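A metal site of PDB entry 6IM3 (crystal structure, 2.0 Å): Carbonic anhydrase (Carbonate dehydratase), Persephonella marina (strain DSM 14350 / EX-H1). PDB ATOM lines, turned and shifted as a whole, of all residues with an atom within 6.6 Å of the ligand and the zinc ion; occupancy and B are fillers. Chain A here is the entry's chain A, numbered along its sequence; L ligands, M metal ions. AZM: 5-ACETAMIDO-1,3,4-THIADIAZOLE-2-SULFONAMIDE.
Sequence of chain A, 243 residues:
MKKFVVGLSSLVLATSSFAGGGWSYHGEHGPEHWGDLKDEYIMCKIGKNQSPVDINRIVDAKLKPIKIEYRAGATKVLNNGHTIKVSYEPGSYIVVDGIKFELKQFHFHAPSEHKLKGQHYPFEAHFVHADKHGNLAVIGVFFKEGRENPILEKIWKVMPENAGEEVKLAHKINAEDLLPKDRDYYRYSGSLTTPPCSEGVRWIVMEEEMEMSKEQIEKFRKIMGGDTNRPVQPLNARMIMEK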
ATOM      1  N   TYR A  25      15.603 -34.840   8.971  1.00  0.00           N
ATOM      2  CA  TYR A  25      16.413 -36.057   8.930  1.00  0.00           C
ATOM      3  C   TYR A  25      15.613 -37.343   8.661  1.00  0.00           C
ATOM      4  O   TYR A  25      16.216 -38.394   8.451  1.00  0.00           O
ATOM      5  CB  TYR A  25      17.269 -36.189  10.226  1.00  0.00           C
ATOM      6  CG  TYR A  25      18.483 -35.278  10.234  1.00  0.00           C
ATOM      7  CD1 TYR A  25      19.460 -35.389   9.209  1.00  0.00           C
ATOM      8  CD2 TYR A  25      18.628 -34.287  11.166  1.00  0.00           C
ATOM      9  CE1 TYR A  25      20.560 -34.529   9.161  1.00  0.00           C
ATOM     10  CE2 TYR A  25      19.765 -33.438  11.167  1.00  0.00           C
ATOM     11  CZ  TYR A  25      20.714 -33.555  10.148  1.00  0.00           C
ATOM     12  OH  TYR A  25      21.832 -32.726  10.114  1.00  0.00           O
ATOM     13  N   SER A  51      28.840 -33.909   0.676  1.00  0.00           N
ATOM     14  CA  SER A  51      29.297 -34.443   1.923  1.00  0.00           C
ATOM     15  C   SER A  51      28.062 -34.855   2.758  1.00  0.00           C
ATOM     16  O   SER A  51      26.975 -34.357   2.533  1.00  0.00           O
ATOM     17  CB  SER A  51      30.044 -33.379   2.733  1.00  0.00           C
ATOM     18  OG  SER A  51      31.185 -32.902   2.031  1.00  0.00           O
ATOM     19  N   THR A  83      20.410 -29.907  15.689  1.00  0.00           N
ATOM     20  CA  THR A  83      21.636 -30.098  16.359  1.00  0.00           C
ATOM     21  C   THR A  83      21.667 -29.180  17.605  1.00  0.00           C
ATOM     22  O   THR A  83      20.750 -28.385  17.818  1.00  0.00           O
ATOM     23  CB  THR A  83      22.836 -29.717  15.417  1.00  0.00           C
ATOM     24  OG1 THR A  83      24.083 -30.119  16.007  1.00  0.00           O
ATOM     25  CG2 THR A  83      22.895 -28.197  15.089  1.00  0.00           C
ATOM     26  N   LYS A  85      24.213 -26.337  18.825  1.00  0.00           N
ATOM     27  CA  LYS A  85      25.176 -25.475  18.174  1.00  0.00           C
ATOM     28  C   LYS A  85      25.734 -24.466  19.165  1.00  0.00           C
ATOM     29  O   LYS A  85      24.971 -23.739  19.810  1.00  0.00           O
ATOM     30  CB  LYS A  85      24.508 -24.749  17.060  1.00  0.00           C
ATOM     31  CG  LYS A  85      25.459 -23.848  16.280  1.00  0.00           C
ATOM     32  CD  LYS A  85      24.751 -22.987  15.248  1.00  0.00           C
ATOM     33  CE  LYS A  85      24.448 -21.629  15.854  1.00  0.00           C
ATOM     34  NZ  LYS A  85      23.776 -20.685  14.920  1.00  0.00           N
ATOM     35  N   GLN A 105      31.264 -21.257  14.768  1.00  0.00           N
ATOM     36  CA  GLN A 105      30.414 -22.110  15.608  1.00  0.00           C
ATOM     37  C   GLN A 105      30.890 -23.565  15.514  1.00  0.00           C
ATOM     38  O   GLN A 105      31.590 -23.937  14.549  1.00  0.00           O
ATOM     39  CB  GLN A 105      28.936 -22.035  15.203  1.00  0.00           C
ATOM     40  CG  GLN A 105      28.596 -22.292  13.736  1.00  0.00           C
ATOM     41  CD  GLN A 105      28.074 -23.697  13.428  1.00  0.00           C
ATOM     42  OE1 GLN A 105      28.302 -24.674  14.168  1.00  0.00           O
ATOM     43  NE2 GLN A 105      27.420 -23.832  12.337  1.00  0.00           N
ATOM     44  N   HIS A 107      29.086 -27.686  16.242  1.00  0.00           N
ATOM     45  CA  HIS A 107      27.846 -28.398  16.460  1.00  0.00           C
ATOM     46  C   HIS A 107      28.111 -29.895  16.347  1.00  0.00           C
ATOM     47  O   HIS A 107      29.240 -30.304  16.044  1.00  0.00           O
ATOM     48  CB  HIS A 107      26.762 -27.892  15.511  1.00  0.00           C
ATOM     49  CG  HIS A 107      27.071 -28.139  14.086  1.00  0.00           C
ATOM     50  ND1 HIS A 107      27.691 -27.211  13.256  1.00  0.00           N
ATOM     51  CD2 HIS A 107      26.916 -29.258  13.352  1.00  0.00           C
ATOM     52  CE1 HIS A 107      27.862 -27.707  12.036  1.00  0.00           C
ATOM     53  NE2 HIS A 107      27.408 -28.941  12.123  1.00  0.00           N
ATOM     54  N   PHE A 108      27.066 -30.668  16.543  1.00  0.00           N
ATOM     55  CA  PHE A 108      27.209 -32.137  16.680  1.00  0.00           C
ATOM     56  C   PHE A 108      26.203 -32.942  15.876  1.00  0.00           C
ATOM     57  O   PHE A 108      25.102 -32.495  15.522  1.00  0.00           O
ATOM     58  CB  PHE A 108      27.097 -32.524  18.144  1.00  0.00           C
ATOM     59  CG  PHE A 108      27.944 -31.699  19.018  1.00  0.00           C
ATOM     60  CD1 PHE A 108      29.323 -31.941  19.092  1.00  0.00           C
ATOM     61  CD2 PHE A 108      27.404 -30.652  19.741  1.00  0.00           C
ATOM     62  CE1 PHE A 108      30.127 -31.195  19.932  1.00  0.00           C
ATOM     63  CE2 PHE A 108      28.198 -29.876  20.541  1.00  0.00           C
ATOM     64  CZ  PHE A 108      29.560 -30.111  20.609  1.00  0.00           C
ATOM     65  N   HIS A 109      26.607 -34.177  15.572  1.00  0.00           N
ATOM     66  CA  HIS A 109      25.729 -35.103  14.927  1.00  0.00           C
ATOM     67  C   HIS A 109      25.890 -36.512  15.550  1.00  0.00           C
ATOM     68  O   HIS A 109      26.978 -36.865  15.995  1.00  0.00           O
ATOM     69  CB  HIS A 109      26.110 -35.265  13.449  1.00  0.00           C
ATOM     70  CG  HIS A 109      26.026 -34.026  12.652  1.00  0.00           C
ATOM     71  ND1 HIS A 109      24.892 -33.647  11.956  1.00  0.00           N
ATOM     72  CD2 HIS A 109      26.969 -33.081  12.386  1.00  0.00           C
ATOM     73  CE1 HIS A 109      25.130 -32.520  11.274  1.00  0.00           C
ATOM     74  NE2 HIS A 109      26.353 -32.197  11.559  1.00  0.00           N
ATOM     75  N   GLU A 113      28.541 -38.471  10.705  1.00  0.00           N
ATOM     76  CA  GLU A 113      28.124 -38.202   9.319  1.00  0.00           C
ATOM     77  C   GLU A 113      29.068 -38.896   8.351  1.00  0.00           C
ATOM     78  O   GLU A 113      28.671 -39.677   7.524  1.00  0.00           O
ATOM     79  CB  GLU A 113      28.086 -36.696   9.035  1.00  0.00           C
ATOM     80  CG  GLU A 113      27.036 -35.988   9.860  1.00  0.00           C
ATOM     81  CD  GLU A 113      26.303 -34.921   9.061  1.00  0.00           C
ATOM     82  OE1 GLU A 113      26.851 -33.800   8.924  1.00  0.00           O
ATOM     83  OE2 GLU A 113      25.204 -35.229   8.540  1.00  0.00           O
ATOM     84  N   GLU A 124      29.988 -37.238  16.085  1.00  0.00           N
ATOM     85  CA  GLU A 124      30.901 -36.426  15.280  1.00  0.00           C
ATOM     86  C   GLU A 124      30.637 -34.912  15.593  1.00  0.00           C
ATOM     87  O   GLU A 124      29.461 -34.454  15.570  1.00  0.00           O
ATOM     88  CB  GLU A 124      30.702 -36.677  13.760  1.00  0.00           C
ATOM     89  CG  GLU A 124      31.700 -35.938  12.840  1.00  0.00           C
ATOM     90  CD  GLU A 124      31.610 -36.327  11.333  1.00  0.00           C
ATOM     91  OE1 GLU A 124      31.063 -37.425  10.990  1.00  0.00           O
ATOM     92  OE2 GLU A 124      32.016 -35.498  10.454  1.00  0.00           O
ATOM     93  N   ALA A 125      31.707 -34.185  15.870  1.00  0.00           N
ATOM     94  CA  ALA A 125      31.656 -32.720  15.975  1.00  0.00           C
ATOM     95  C   ALA A 125      32.166 -31.976  14.723  1.00  0.00           C
ATOM     96  O   ALA A 125      33.110 -32.428  14.062  1.00  0.00           O
ATOM     97  CB  ALA A 125      32.468 -32.281  17.161  1.00  0.00           C
ATOM     98  N   HIS A 126      31.523 -30.881  14.395  1.00  0.00           N
ATOM     99  CA  HIS A 126      31.909 -30.021  13.258  1.00  0.00           C
ATOM    100  C   HIS A 126      32.206 -28.617  13.714  1.00  0.00           C
ATOM    101  O   HIS A 126      31.373 -28.008  14.361  1.00  0.00           O
ATOM    102  CB  HIS A 126      30.805 -29.932  12.242  1.00  0.00           C
ATOM    103  CG  HIS A 126      30.557 -31.199  11.512  1.00  0.00           C
ATOM    104  ND1 HIS A 126      29.382 -31.446  10.805  1.00  0.00           N
ATOM    105  CD2 HIS A 126      31.309 -32.306  11.401  1.00  0.00           C
ATOM    106  CE1 HIS A 126      29.489 -32.672  10.278  1.00  0.00           C
ATOM    107  NE2 HIS A 126      30.647 -33.184  10.621  1.00  0.00           N
ATOM    108  N   PHE A 127      33.378 -28.128  13.323  1.00  0.00           N
ATOM    109  CA  PHE A 127      33.835 -26.821  13.644  1.00  0.00           C
ATOM    110  C   PHE A 127      33.854 -25.988  12.359  1.00  0.00           C
ATOM    111  O   PHE A 127      34.605 -26.314  11.431  1.00  0.00           O
ATOM    112  CB  PHE A 127      35.236 -26.842  14.327  1.00  0.00           C
ATOM    113  CG  PHE A 127      35.288 -27.668  15.574  1.00  0.00           C
ATOM    114  CD1 PHE A 127      35.316 -29.039  15.520  1.00  0.00           C
ATOM    115  CD2 PHE A 127      35.246 -27.048  16.823  1.00  0.00           C
ATOM    116  CE1 PHE A 127      35.318 -29.811  16.706  1.00  0.00           C
ATOM    117  CE2 PHE A 127      35.238 -27.803  17.955  1.00  0.00           C
ATOM    118  CZ  PHE A 127      35.270 -29.191  17.902  1.00  0.00           C
ATOM    119  N   VAL A 128      32.938 -25.015  12.290  1.00  0.00           N
ATOM    120  CA  VAL A 128      32.565 -24.339  11.059  1.00  0.00           C
ATOM    121  C   VAL A 128      33.255 -22.958  10.976  1.00  0.00           C
ATOM    122  O   VAL A 128      33.144 -22.168  11.900  1.00  0.00           O
ATOM    123  CB  VAL A 128      31.105 -24.180  10.888  1.00  0.00           C
ATOM    124  CG1 VAL A 128      30.739 -23.488   9.548  1.00  0.00           C
ATOM    125  CG2 VAL A 128      30.380 -25.541  10.967  1.00  0.00           C
ATOM    126  N   LEU A 136      33.957 -21.510   3.077  1.00  0.00           N
ATOM    127  CA  LEU A 136      33.832 -22.288   4.343  1.00  0.00           C
ATOM    128  C   LEU A 136      34.817 -23.432   4.443  1.00  0.00           C
ATOM    129  O   LEU A 136      35.211 -24.034   3.418  1.00  0.00           O
ATOM    130  CB  LEU A 136      32.398 -22.838   4.382  1.00  0.00           C
ATOM    131  CG  LEU A 136      31.258 -21.844   4.303  1.00  0.00           C
ATOM    132  CD1 LEU A 136      29.944 -22.603   4.269  1.00  0.00           C
ATOM    133  CD2 LEU A 136      31.240 -20.888   5.503  1.00  0.00           C
ATOM    134  N   VAL A 138      35.347 -26.700   7.235  1.00  0.00           N
ATOM    135  CA  VAL A 138      34.803 -27.447   8.411  1.00  0.00           C
ATOM    136  C   VAL A 138      35.795 -28.521   8.867  1.00  0.00           C
ATOM    137  O   VAL A 138      36.311 -29.259   7.999  1.00  0.00           O
ATOM    138  CB  VAL A 138      33.457 -28.101   8.107  1.00  0.00           C
ATOM    139  CG1 VAL A 138      32.875 -28.676   9.372  1.00  0.00           C
ATOM    140  CG2 VAL A 138      32.477 -27.114   7.501  1.00  0.00           C
ATOM    141  N   SER A 191      30.828 -30.334   0.690  1.00  0.00           N
ATOM    142  CA  SER A 191      29.622 -29.500   0.801  1.00  0.00           C
ATOM    143  C   SER A 191      29.180 -29.364   2.224  1.00  0.00           C
ATOM    144  O   SER A 191      29.609 -30.110   3.111  1.00  0.00           O
ATOM    145  CB  SER A 191      28.447 -30.085  -0.006  1.00  0.00           C
ATOM    146  OG  SER A 191      27.766 -31.163   0.652  1.00  0.00           O
ATOM    147  N   LEU A 192      28.258 -28.433   2.449  1.00  0.00           N
ATOM    148  CA  LEU A 192      27.518 -28.415   3.710  1.00  0.00           C
ATOM    149  C   LEU A 192      26.615 -29.646   3.733  1.00  0.00           C
ATOM    150  O   LEU A 192      26.204 -30.142   2.662  1.00  0.00           O
ATOM    151  CB  LEU A 192      26.694 -27.133   3.841  1.00  0.00           C
ATOM    152  CG  LEU A 192      27.556 -25.876   3.945  1.00  0.00           C
ATOM    153  CD1 LEU A 192      26.618 -24.656   4.043  1.00  0.00           C
ATOM    154  CD2 LEU A 192      28.500 -25.891   5.103  1.00  0.00           C
ATOM    155  N   THR A 193      26.408 -30.206   4.927  1.00  0.00           N
ATOM    156  CA  THR A 193      25.637 -31.456   5.043  1.00  0.00           C
ATOM    157  C   THR A 193      24.114 -31.275   5.355  1.00  0.00           C
ATOM    158  O   THR A 193      23.405 -32.235   5.530  1.00  0.00           O
ATOM    159  CB  THR A 193      26.217 -32.414   6.075  1.00  0.00           C
ATOM    160  OG1 THR A 193      26.089 -31.928   7.396  1.00  0.00           O
ATOM    161  CG2 THR A 193      27.693 -32.684   5.765  1.00  0.00           C
ATOM    162  N   THR A 194      23.687 -30.018   5.437  1.00  0.00           N
ATOM    163  CA  THR A 194      22.278 -29.698   5.522  1.00  0.00           C
ATOM    164  C   THR A 194      21.935 -28.678   4.451  1.00  0.00           C
ATOM    165  O   THR A 194      22.837 -27.934   3.990  1.00  0.00           O
ATOM    166  CB  THR A 194      21.915 -29.100   6.875  1.00  0.00           C
ATOM    167  OG1 THR A 194      22.662 -27.894   7.070  1.00  0.00           O
ATOM    168  CG2 THR A 194      22.291 -30.050   7.963  1.00  0.00           C
ATOM    169  N   PRO A 195      20.648 -28.631   4.009  1.00  0.00           N
ATOM    170  CA  PRO A 195      20.259 -27.768   2.852  1.00  0.00           C
ATOM    171  C   PRO A 195      20.620 -26.356   3.148  1.00  0.00           C
ATOM    172  O   PRO A 195      20.543 -25.963   4.295  1.00  0.00           O
ATOM    173  CB  PRO A 195      18.719 -27.959   2.786  1.00  0.00           C
ATOM    174  CG  PRO A 195      18.512 -29.324   3.318  1.00  0.00           C
ATOM    175  CD  PRO A 195      19.506 -29.460   4.449  1.00  0.00           C
ATOM    176  N   PRO A 196      21.170 -25.604   2.211  1.00  0.00           N
ATOM    177  CA  PRO A 196      21.209 -25.902   0.764  1.00  0.00           C
ATOM    178  C   PRO A 196      22.340 -26.784   0.255  1.00  0.00           C
ATOM    179  O   PRO A 196      22.451 -26.972  -0.958  1.00  0.00           O
ATOM    180  CB  PRO A 196      21.316 -24.492   0.142  1.00  0.00           C
ATOM    181  CG  PRO A 196      22.020 -23.636   1.156  1.00  0.00           C
ATOM    182  CD  PRO A 196      21.704 -24.243   2.532  1.00  0.00           C
ATOM    183  N   VAL A 201      33.249 -26.410  -0.226  1.00  0.00           N
ATOM    184  CA  VAL A 201      33.609 -26.461   1.222  1.00  0.00           C
ATOM    185  C   VAL A 201      34.859 -27.296   1.435  1.00  0.00           C
ATOM    186  O   VAL A 201      34.956 -28.408   0.940  1.00  0.00           O
ATOM    187  CB  VAL A 201      32.465 -27.041   2.058  1.00  0.00           C
ATOM    188  CG1 VAL A 201      32.835 -27.131   3.568  1.00  0.00           C
ATOM    189  CG2 VAL A 201      31.266 -26.176   1.897  1.00  0.00           C
ATOM    190  N   TRP A 203      36.840 -29.676   3.583  1.00  0.00           N
ATOM    191  CA  TRP A 203      36.663 -30.604   4.717  1.00  0.00           C
ATOM    192  C   TRP A 203      37.994 -31.092   5.179  1.00  0.00           C
ATOM    193  O   TRP A 203      38.827 -31.585   4.426  1.00  0.00           O
ATOM    194  CB  TRP A 203      35.768 -31.798   4.329  1.00  0.00           C
ATOM    195  CG  TRP A 203      34.359 -31.511   4.445  1.00  0.00           C
ATOM    196  CD1 TRP A 203      33.532 -31.074   3.479  1.00  0.00           C
ATOM    197  CD2 TRP A 203      33.591 -31.516   5.660  1.00  0.00           C
ATOM    198  NE1 TRP A 203      32.299 -30.814   4.003  1.00  0.00           N
ATOM    199  CE2 TRP A 203      32.306 -31.094   5.324  1.00  0.00           C
ATOM    200  CE3 TRP A 203      33.854 -31.939   6.950  1.00  0.00           C
ATOM    201  CZ2 TRP A 203      31.277 -31.046   6.260  1.00  0.00           C
ATOM    202  CZ3 TRP A 203      32.847 -31.860   7.885  1.00  0.00           C
ATOM    203  CH2 TRP A 203      31.589 -31.416   7.528  1.00  0.00           C
HETATM  204  C1  AZM L   1      26.753 -27.546   8.158  1.00  0.00           C
HETATM  205  C2  AZM L   1      25.593 -25.388   8.065  1.00  0.00           C
HETATM  206  C3  AZM L   1      25.750 -23.054   8.561  1.00  0.00           C
HETATM  207  C4  AZM L   1      24.978 -21.753   8.619  1.00  0.00           C
HETATM  208  N1  AZM L   1      27.029 -30.174   8.854  1.00  0.00           N
HETATM  209  N2  AZM L   1      24.893 -26.401   7.490  1.00  0.00           N
HETATM  210  N3  AZM L   1      25.552 -27.645   7.507  1.00  0.00           N
HETATM  211  N4  AZM L   1      25.110 -24.101   8.041  1.00  0.00           N
HETATM  212  O1  AZM L   1      28.205 -29.155   7.024  1.00  0.00           O
HETATM  213  O2  AZM L   1      28.842 -28.419   9.151  1.00  0.00           O
HETATM  214  O3  AZM L   1      26.891 -23.102   8.930  1.00  0.00           O
HETATM  215  S1  AZM L   1      27.796 -28.823   8.337  1.00  0.00           S
HETATM  216  S2  AZM L   1      27.144 -25.899   8.727  1.00  0.00           S
HETATM  217 ZN    ZN M   1      27.499 -30.513  10.775  1.00  0.00          ZN
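Gln 105 touches the ligand. OE1 of Glu 113 touches N1 of the ligand, at 3.6 Å. CG2 of Val 128 touches O2 of the ligand, at 3.7 Å. Leu 192 touches the ligand. Trp 203 touches the ligand. Hydrophobic or aromatic side chains that line the ligand: His 107, His 109, His 126, Val 128, Leu 192 and Trp 203.
Residues that only touch the zinc ion: Glu 113 and Thr 193. Five residues have an atom within 4 Å of the zinc ion: His 107, His 109, Glu 113, His 126 and Thr 193. The nearest printed residue that does not touch the zinc ion is Trp 203 (5.3 Å).
OE1 of Gln 105 is in hydrogen-bond range of ND1 of His 107 (2.8 Å). NE2 of His 126 lies within hydrogen-bond range of OE2 of Glu 124. NE2 of His 109 sits close to OE1 of Glu 113 (3.1 Å). The backbone NH (N) of His 109 lies within hydrogen-bond range of the backbone carbonyl oxygen (O) of Glu 124 (2.9 Å). The side-chain carboxylate of Glu 113 is in hydrogen-bond range of the side-chain hydroxyl of Thr 193. The backbone carbonyl oxygen (O) of Gln 105 is in hydrogen-bond range of the backbone NH (N) of Val 128. N of Glu 113 sits at hydrogen-bond distance from OE1 of Glu 124 (2.7 Å). NE1 of Trp 203 lies within hydrogen-bond range of O of Ser 191 (2.9 Å).
N1 of the ligand binds the zinc ion (2.0 Å). A ring nitrogen (NE2) of His 107 binds the zinc ion (2.1 Å). ND1 of His 126 is bound to the zinc ion. The zinc ion is bound by NE2 of His 109 (2.2 Å).
The backbone NH of Thr 193 is in hydrogen-bond range of an oxygen (O1) of the ligand (3.0 Å). A nitrogen (N1) of the ligand lies close to the side-chain hydroxyl of Thr 193 (2.5 Å). The side-chain hydroxyl (OG1) of Thr 194 sits at hydrogen-bond distance from a nitrogen (N2) of the ligand.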
